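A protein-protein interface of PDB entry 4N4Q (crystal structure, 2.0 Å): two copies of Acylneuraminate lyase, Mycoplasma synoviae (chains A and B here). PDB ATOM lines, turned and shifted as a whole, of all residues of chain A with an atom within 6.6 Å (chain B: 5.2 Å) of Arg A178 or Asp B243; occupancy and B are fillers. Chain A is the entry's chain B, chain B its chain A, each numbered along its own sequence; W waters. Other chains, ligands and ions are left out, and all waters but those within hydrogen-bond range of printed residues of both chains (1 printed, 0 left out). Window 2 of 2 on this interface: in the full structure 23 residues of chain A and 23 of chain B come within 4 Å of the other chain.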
ATOM      1  N   THR A 151     -18.857  14.418  26.386  1.00  0.00           N
ATOM      2  CA  THR A 151     -18.103  14.649  25.162  1.00  0.00           C
ATOM      3  C   THR A 151     -18.433  13.545  24.163  1.00  0.00           C
ATOM      4  O   THR A 151     -18.675  13.833  22.984  1.00  0.00           O
ATOM      5  CB  THR A 151     -16.578  14.712  25.416  1.00  0.00           C
ATOM      6  OG1 THR A 151     -16.290  15.789  26.316  1.00  0.00           O
ATOM      7  CG2 THR A 151     -15.813  14.957  24.111  1.00  0.00           C
ATOM      8  N   LEU A 173     -14.685  26.783  28.591  1.00  0.00           N
ATOM      9  CA  LEU A 173     -13.670  26.643  27.561  1.00  0.00           C
ATOM     10  C   LEU A 173     -12.914  25.312  27.624  1.00  0.00           C
ATOM     11  O   LEU A 173     -12.237  24.936  26.664  1.00  0.00           O
ATOM     12  CB  LEU A 173     -12.768  27.879  27.518  1.00  0.00           C
ATOM     13  CG  LEU A 173     -13.652  29.123  27.274  1.00  0.00           C
ATOM     14  CD1 LEU A 173     -12.987  30.471  27.529  1.00  0.00           C
ATOM     15  CD2 LEU A 173     -14.276  29.086  25.879  1.00  0.00           C
ATOM     16  N   PHE A 174     -13.070  24.588  28.737  1.00  0.00           N
ATOM     17  CA  PHE A 174     -12.556  23.225  28.866  1.00  0.00           C
ATOM     18  C   PHE A 174     -13.317  22.255  27.967  1.00  0.00           C
ATOM     19  O   PHE A 174     -12.707  21.558  27.153  1.00  0.00           O
ATOM     20  CB  PHE A 174     -12.563  22.761  30.340  1.00  0.00           C
ATOM     21  CG  PHE A 174     -11.898  21.431  30.556  1.00  0.00           C
ATOM     22  CD1 PHE A 174     -10.582  21.220  30.153  1.00  0.00           C
ATOM     23  CD2 PHE A 174     -12.590  20.381  31.150  1.00  0.00           C
ATOM     24  CE1 PHE A 174      -9.976  19.990  30.327  1.00  0.00           C
ATOM     25  CE2 PHE A 174     -11.982  19.146  31.330  1.00  0.00           C
ATOM     26  CZ  PHE A 174     -10.668  18.955  30.920  1.00  0.00           C
ATOM     27  N   ALA A 175     -14.649  22.230  28.085  1.00  0.00           N
ATOM     28  CA  ALA A 175     -15.493  21.461  27.170  1.00  0.00           C
ATOM     29  C   ALA A 175     -15.170  21.791  25.735  1.00  0.00           C
ATOM     30  O   ALA A 175     -15.156  20.901  24.889  1.00  0.00           O
ATOM     31  CB  ALA A 175     -16.967  21.703  27.422  1.00  0.00           C
ATOM     32  N   PHE A 176     -14.933  23.069  25.455  1.00  0.00           N
ATOM     33  CA  PHE A 176     -14.500  23.486  24.113  1.00  0.00           C
ATOM     34  C   PHE A 176     -13.139  22.871  23.733  1.00  0.00           C
ATOM     35  O   PHE A 176     -13.036  22.193  22.722  1.00  0.00           O
ATOM     36  CB  PHE A 176     -14.502  25.009  23.925  1.00  0.00           C
ATOM     37  CG  PHE A 176     -14.202  25.435  22.494  1.00  0.00           C
ATOM     38  CD1 PHE A 176     -15.056  25.085  21.455  1.00  0.00           C
ATOM     39  CD2 PHE A 176     -13.042  26.144  22.187  1.00  0.00           C
ATOM     40  CE1 PHE A 176     -14.764  25.450  20.133  1.00  0.00           C
ATOM     41  CE2 PHE A 176     -12.756  26.520  20.873  1.00  0.00           C
ATOM     42  CZ  PHE A 176     -13.608  26.164  19.854  1.00  0.00           C
ATOM     43  N   GLU A 177     -12.105  23.079  24.546  1.00  0.00           N
ATOM     44  CA  GLU A 177     -10.826  22.397  24.269  1.00  0.00           C
ATOM     45  C   GLU A 177     -11.055  20.895  23.987  1.00  0.00           C
ATOM     46  O   GLU A 177     -10.542  20.358  22.981  1.00  0.00           O
ATOM     47  CB  GLU A 177      -9.823  22.640  25.405  1.00  0.00           C
ATOM     48  CG  GLU A 177      -8.481  21.906  25.271  1.00  0.00           C
ATOM     49  CD  GLU A 177      -8.590  20.418  25.601  1.00  0.00           C
ATOM     50  OE1 GLU A 177      -9.179  20.067  26.650  1.00  0.00           O
ATOM     51  OE2 GLU A 177      -8.068  19.598  24.823  1.00  0.00           O
ATOM     52  N   ARG A 178     -11.873  20.228  24.815  1.00  0.00           N
ATOM     53  CA  ARG A 178     -12.114  18.775  24.633  1.00  0.00           C
ATOM     54  C   ARG A 178     -12.777  18.405  23.304  1.00  0.00           C
ATOM     55  O   ARG A 178     -12.437  17.368  22.700  1.00  0.00           O
ATOM     56  CB  ARG A 178     -12.899  18.145  25.811  1.00  0.00           C
ATOM     57  CG  ARG A 178     -12.242  18.312  27.199  1.00  0.00           C
ATOM     58  CD  ARG A 178     -11.172  17.248  27.535  1.00  0.00           C
ATOM     59  NE  ARG A 178      -9.903  17.426  26.830  1.00  0.00           N
ATOM     60  CZ  ARG A 178      -9.047  16.437  26.541  1.00  0.00           C
ATOM     61  NH1 ARG A 178      -7.926  16.702  25.878  1.00  0.00           N
ATOM     62  NH2 ARG A 178      -9.316  15.182  26.897  1.00  0.00           N
ATOM     63  N   LEU A 179     -13.739  19.210  22.858  1.00  0.00           N
ATOM     64  CA  LEU A 179     -14.404  18.932  21.585  1.00  0.00           C
ATOM     65  C   LEU A 179     -13.448  19.080  20.406  1.00  0.00           C
ATOM     66  O   LEU A 179     -13.434  18.249  19.520  1.00  0.00           O
ATOM     67  CB  LEU A 179     -15.669  19.777  21.392  1.00  0.00           C
ATOM     68  CG  LEU A 179     -16.859  19.383  22.270  1.00  0.00           C
ATOM     69  CD1 LEU A 179     -18.022  20.373  22.105  1.00  0.00           C
ATOM     70  CD2 LEU A 179     -17.344  17.964  22.000  1.00  0.00           C
ATOM     71  N   MET A 180     -12.623  20.113  20.427  1.00  0.00           N
ATOM     72  CA  MET A 180     -11.648  20.333  19.350  1.00  0.00           C
ATOM     73  C   MET A 180     -10.612  19.198  19.312  1.00  0.00           C
ATOM     74  O   MET A 180     -10.113  18.838  18.257  1.00  0.00           O
ATOM     75  CB  MET A 180     -10.974  21.684  19.532  1.00  0.00           C
ATOM     76  CG  MET A 180     -11.945  22.856  19.420  1.00  0.00           C
ATOM     77  SD  MET A 180     -12.500  23.116  17.717  1.00  0.00           S
ATOM     78  CE  MET A 180     -10.961  23.504  16.873  1.00  0.00           C
ATOM     79  N   SER A 181     -10.317  18.626  20.476  1.00  0.00           N
ATOM     80  CA  SER A 181      -9.410  17.490  20.554  1.00  0.00           C
ATOM     81  C   SER A 181     -10.052  16.217  19.983  1.00  0.00           C
ATOM     82  O   SER A 181      -9.417  15.486  19.227  1.00  0.00           O
ATOM     83  CB  SER A 181      -8.960  17.266  22.001  1.00  0.00           C
ATOM     84  OG  SER A 181      -8.240  16.047  22.128  1.00  0.00           O
ATOM     85  N   LYS A 182     -11.313  15.965  20.330  1.00  0.00           N
ATOM     86  CA  LYS A 182     -11.986  14.730  19.953  1.00  0.00           C
ATOM     87  C   LYS A 182     -12.503  14.764  18.523  1.00  0.00           C
ATOM     88  O   LYS A 182     -12.604  13.717  17.875  1.00  0.00           O
ATOM     89  CB  LYS A 182     -13.143  14.452  20.920  1.00  0.00           C
ATOM     90  CG  LYS A 182     -13.773  13.066  20.797  1.00  0.00           C
ATOM     91  CD  LYS A 182     -13.227  12.088  21.843  1.00  0.00           C
ATOM     92  CE  LYS A 182     -13.530  10.640  21.443  1.00  0.00           C
ATOM     93  NZ  LYS A 182     -14.958  10.472  20.986  1.00  0.00           N
ATOM     94  N   TYR A 183     -12.833  15.960  18.025  1.00  0.00           N
ATOM     95  CA  TYR A 183     -13.507  16.078  16.735  1.00  0.00           C
ATOM     96  C   TYR A 183     -12.859  17.122  15.833  1.00  0.00           C
ATOM     97  O   TYR A 183     -13.477  18.127  15.518  1.00  0.00           O
ATOM     98  CB  TYR A 183     -14.996  16.421  16.914  1.00  0.00           C
ATOM     99  CG  TYR A 183     -15.756  15.527  17.865  1.00  0.00           C
ATOM    100  CD1 TYR A 183     -16.190  14.267  17.479  1.00  0.00           C
ATOM    101  CD2 TYR A 183     -16.048  15.951  19.153  1.00  0.00           C
ATOM    102  CE1 TYR A 183     -16.896  13.445  18.370  1.00  0.00           C
ATOM    103  CE2 TYR A 183     -16.744  15.139  20.039  1.00  0.00           C
ATOM    104  CZ  TYR A 183     -17.165  13.894  19.641  1.00  0.00           C
ATOM    105  OH  TYR A 183     -17.850  13.095  20.529  1.00  0.00           O
ATOM    106  N   THR B 238      -1.619  21.123  24.433  1.00  0.00           N
ATOM    107  CA  THR B 238      -2.726  21.278  25.384  1.00  0.00           C
ATOM    108  C   THR B 238      -3.671  20.078  25.391  1.00  0.00           C
ATOM    109  O   THR B 238      -4.142  19.658  26.468  1.00  0.00           O
ATOM    110  CB  THR B 238      -3.507  22.574  25.109  1.00  0.00           C
ATOM    111  OG1 THR B 238      -2.667  23.690  25.423  1.00  0.00           O
ATOM    112  CG2 THR B 238      -4.812  22.652  25.931  1.00  0.00           C
ATOM    113  N   HIS B 239      -3.949  19.528  24.209  1.00  0.00           N
ATOM    114  CA  HIS B 239      -4.831  18.382  24.101  1.00  0.00           C
ATOM    115  C   HIS B 239      -4.233  17.166  24.807  1.00  0.00           C
ATOM    116  O   HIS B 239      -4.955  16.460  25.511  1.00  0.00           O
ATOM    117  CB  HIS B 239      -5.146  18.028  22.643  1.00  0.00           C
ATOM    118  CG  HIS B 239      -5.927  19.078  21.911  1.00  0.00           C
ATOM    119  ND1 HIS B 239      -6.971  19.767  22.484  1.00  0.00           N
ATOM    120  CD2 HIS B 239      -5.819  19.545  20.645  1.00  0.00           C
ATOM    121  CE1 HIS B 239      -7.482  20.606  21.599  1.00  0.00           C
ATOM    122  NE2 HIS B 239      -6.795  20.499  20.479  1.00  0.00           N
ATOM    123  N   THR B 240      -2.938  16.916  24.567  1.00  0.00           N
ATOM    124  CA  THR B 240      -2.174  15.883  25.288  1.00  0.00           C
ATOM    125  C   THR B 240      -2.120  16.150  26.789  1.00  0.00           C
ATOM    126  O   THR B 240      -2.291  15.240  27.597  1.00  0.00           O
ATOM    127  CB  THR B 240      -0.718  15.716  24.745  1.00  0.00           C
ATOM    128  OG1 THR B 240      -0.745  15.644  23.315  1.00  0.00           O
ATOM    129  CG2 THR B 240      -0.084  14.430  25.296  1.00  0.00           C
ATOM    130  N   TYR B 241      -1.868  17.390  27.172  1.00  0.00           N
ATOM    131  CA  TYR B 241      -1.842  17.692  28.590  1.00  0.00           C
ATOM    132  C   TYR B 241      -3.197  17.428  29.251  1.00  0.00           C
ATOM    133  O   TYR B 241      -3.270  16.941  30.379  1.00  0.00           O
ATOM    134  CB  TYR B 241      -1.369  19.107  28.856  1.00  0.00           C
ATOM    135  CG  TYR B 241      -0.859  19.236  30.253  1.00  0.00           C
ATOM    136  CD1 TYR B 241       0.449  18.861  30.562  1.00  0.00           C
ATOM    137  CD2 TYR B 241      -1.693  19.670  31.290  1.00  0.00           C
ATOM    138  CE1 TYR B 241       0.922  18.946  31.859  1.00  0.00           C
ATOM    139  CE2 TYR B 241      -1.218  19.761  32.593  1.00  0.00           C
ATOM    140  CZ  TYR B 241       0.088  19.389  32.867  1.00  0.00           C
ATOM    141  OH  TYR B 241       0.584  19.465  34.149  1.00  0.00           O
ATOM    142  N   ASN B 242      -4.280  17.712  28.539  1.00  0.00           N
ATOM    143  CA  ASN B 242      -5.592  17.563  29.156  1.00  0.00           C
ATOM    144  C   ASN B 242      -6.085  16.129  29.107  1.00  0.00           C
ATOM    145  O   ASN B 242      -6.886  15.718  29.952  1.00  0.00           O
ATOM    146  CB  ASN B 242      -6.605  18.566  28.589  1.00  0.00           C
ATOM    147  CG  ASN B 242      -6.271  20.011  28.963  1.00  0.00           C
ATOM    148  OD1 ASN B 242      -5.264  20.289  29.618  1.00  0.00           O
ATOM    149  ND2 ASN B 242      -7.111  20.938  28.529  1.00  0.00           N
ATOM    150  N   ASP B 243      -5.585  15.351  28.145  1.00  0.00           N
ATOM    151  CA  ASP B 243      -5.791  13.906  28.204  1.00  0.00           C
ATOM    152  C   ASP B 243      -5.112  13.371  29.462  1.00  0.00           C
ATOM    153  O   ASP B 243      -5.680  12.536  30.168  1.00  0.00           O
ATOM    154  CB  ASP B 243      -5.212  13.189  26.983  1.00  0.00           C
ATOM    155  CG  ASP B 243      -5.996  13.440  25.718  1.00  0.00           C
ATOM    156  OD1 ASP B 243      -7.090  14.041  25.788  1.00  0.00           O
ATOM    157  OD2 ASP B 243      -5.514  13.005  24.647  1.00  0.00           O
ATOM    158  N   TYR B 244      -3.904  13.868  29.729  1.00  0.00           N
ATOM    159  CA  TYR B 244      -3.117  13.429  30.889  1.00  0.00           C
ATOM    160  C   TYR B 244      -3.826  13.793  32.194  1.00  0.00           C
ATOM    161  O   TYR B 244      -3.881  12.965  33.124  1.00  0.00           O
ATOM    162  CB  TYR B 244      -1.704  14.030  30.851  1.00  0.00           C
ATOM    163  CG  TYR B 244      -1.100  14.369  32.212  1.00  0.00           C
ATOM    164  CD1 TYR B 244      -0.647  13.367  33.090  1.00  0.00           C
ATOM    165  CD2 TYR B 244      -0.964  15.701  32.609  1.00  0.00           C
ATOM    166  CE1 TYR B 244      -0.084  13.709  34.344  1.00  0.00           C
ATOM    167  CE2 TYR B 244      -0.403  16.040  33.845  1.00  0.00           C
ATOM    168  CZ  TYR B 244       0.027  15.037  34.705  1.00  0.00           C
ATOM    169  OH  TYR B 244       0.586  15.400  35.903  1.00  0.00           O
ATOM    170  N   VAL B 245      -4.334  15.027  32.269  1.00  0.00           N
ATOM    171  CA  VAL B 245      -5.026  15.479  33.486  1.00  0.00           C
ATOM    172  C   VAL B 245      -6.257  14.622  33.796  1.00  0.00           C
ATOM    173  O   VAL B 245      -6.404  14.161  34.933  1.00  0.00           O
ATOM    174  CB  VAL B 245      -5.337  17.001  33.497  1.00  0.00           C
ATOM    175  CG1 VAL B 245      -6.097  17.387  34.769  1.00  0.00           C
ATOM    176  CG2 VAL B 245      -4.034  17.790  33.419  1.00  0.00           C
ATOM    177  N   LEU B 246      -7.109  14.364  32.803  1.00  0.00           N
ATOM    178  CA  LEU B 246      -8.302  13.504  33.021  1.00  0.00           C
ATOM    179  C   LEU B 246      -7.967  12.031  33.305  1.00  0.00           C
ATOM    180  O   LEU B 246      -8.674  11.343  34.066  1.00  0.00           O
ATOM    181  CB  LEU B 246      -9.286  13.600  31.855  1.00  0.00           C
ATOM    182  CG  LEU B 246      -9.985  14.954  31.695  1.00  0.00           C
ATOM    183  CD1 LEU B 246     -11.012  14.864  30.561  1.00  0.00           C
ATOM    184  CD2 LEU B 246     -10.639  15.405  33.012  1.00  0.00           C
ATOM    185  N   ASP B 247      -6.878  11.575  32.704  1.00  0.00           N
ATOM    186  CA  ASP B 247      -6.307  10.280  33.006  1.00  0.00           C
ATOM    187  C   ASP B 247      -5.818  10.203  34.449  1.00  0.00           C
ATOM    188  O   ASP B 247      -6.210   9.301  35.172  1.00  0.00           O
ATOM    189  CB  ASP B 247      -5.184   9.942  32.008  1.00  0.00           C
ATOM    190  CG  ASP B 247      -5.666   9.065  30.842  1.00  0.00           C
ATOM    191  OD1 ASP B 247      -6.877   8.828  30.709  1.00  0.00           O
ATOM    192  OD2 ASP B 247      -4.825   8.600  30.051  1.00  0.00           O
ATOM    193  N   LEU B 248      -4.982  11.154  34.863  1.00  0.00           N
ATOM    194  CA  LEU B 248      -4.454  11.233  36.235  1.00  0.00           C
ATOM    195  C   LEU B 248      -5.579  11.168  37.283  1.00  0.00           C
ATOM    196  O   LEU B 248      -5.514  10.368  38.222  1.00  0.00           O
ATOM    197  CB  LEU B 248      -3.583  12.492  36.416  1.00  0.00           C
ATOM    198  CG  LEU B 248      -3.007  12.910  37.780  1.00  0.00           C
ATOM    199  CD1 LEU B 248      -1.909  11.998  38.280  1.00  0.00           C
ATOM    200  CD2 LEU B 248      -2.490  14.337  37.749  1.00  0.00           C
ATOM    201  N   TYR B 294       2.467   9.281  29.204  1.00  0.00           N
ATOM    202  CA  TYR B 294       2.636  10.738  29.223  1.00  0.00           C
ATOM    203  C   TYR B 294       3.973  11.255  29.704  1.00  0.00           C
ATOM    204  O   TYR B 294       4.340  12.376  29.384  1.00  0.00           O
ATOM    205  CB  TYR B 294       1.538  11.394  30.068  1.00  0.00           C
ATOM    206  CG  TYR B 294       0.129  11.119  29.600  1.00  0.00           C
ATOM    207  CD1 TYR B 294      -0.402  11.780  28.490  1.00  0.00           C
ATOM    208  CD2 TYR B 294      -0.678  10.200  30.271  1.00  0.00           C
ATOM    209  CE1 TYR B 294      -1.689  11.531  28.060  1.00  0.00           C
ATOM    210  CE2 TYR B 294      -1.970   9.943  29.847  1.00  0.00           C
ATOM    211  CZ  TYR B 294      -2.473  10.613  28.743  1.00  0.00           C
ATOM    212  OH  TYR B 294      -3.761  10.369  28.320  1.00  0.00           O
HETATM  213  O   HOH W   1      -9.114  13.999  23.654  1.00  0.00           O
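O of His B239 lies within hydrogen-bond range of NH1 of Arg A178 (3.0 Å). OE2 of Glu A177 sits at hydrogen-bond distance from ND1 of His B239 (2.6 Å). The side-chain amide nitrogen (ND2) of Asn B242 sits at hydrogen-bond distance from the side-chain carboxylate (OE1) of Glu A177 (2.9 Å). The side-chain carboxylate of Asp B243 lies within salt-bridge range of the guanidinium group of Arg A178, 2.7 Å away.
The side-chain hydroxyl (OH) of Tyr B294 sits at hydrogen-bond distance from the backbone carbonyl oxygen (O) of Asp B243. O of Thr B238 sits close to OD1 of Asn B242 (3.4 Å). The guanidinium group (NE) of Arg A178 is in salt-bridge range of the side-chain carboxylate (OE1) of Glu A177 (2.7 Å).
Phe A174 touches Asn B242. Glu A177 touches Thr B238. Arg A178 touches Asn B242 (NH1 to CB, 3.5 Å). Leu B246 touches Arg A178. ND1 of His B239 touches CB of Ser A181 (3.2 Å).
Of chain B, only His B239 (3.0 Å), Asn B242 (3.5 Å), Asp B243 (2.7 Å) and Leu B246 (3.9 Å) come within 4 Å of Arg A178. Printed residues of chain A within 4 Å of Asp B243: Arg A178. Of the printed residues of chain A, Asn B242 touches Phe A174 (3.5 Å), Glu A177 (2.9 Å) and Arg A178 (3.5 Å). Printed residues of chain B within 4 Å of Phe A174: Asn B242 (3.5 Å). Of the printed residues of chain B, Ser A181 touches His B239. The nearest residue of chain A that does not touch Asp B243 is Ser A181 (4.3 Å). The nearest printed residue of chain A that does not touch Thr B238 is Arg A178 (4.8 Å).
Of the 12 printed residues of chain B, 5 touch a printed residue of chain A. Hydrophobic or aromatic side chains of chain B within 4 Å of the printed part of chain A: His B239 and Leu B246. Hydrophobic or aromatic side chains of chain A within 4 Å of the printed part of chain B: Phe A174. Among the printed residues, Asp or Glu carboxylates within 4 Å of a Lys or Arg side-chain nitrogen of the other chain: Arg A178 with Asp B243 (2.7 Å).
No position is printed for both chains. Of the 9 pairs that touch across the chains among the printed residues, none has its exchanged pair printed and touching as well.
Water W1 lies within hydrogen-bond range of the side-chain hydroxyl (OG) of Ser A181 (2.7 Å), the side-chain carboxylate (OD1) of Asp B243 (2.9 Å) and the guanidinium group (NH2) of Arg A178 (3.5 Å).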
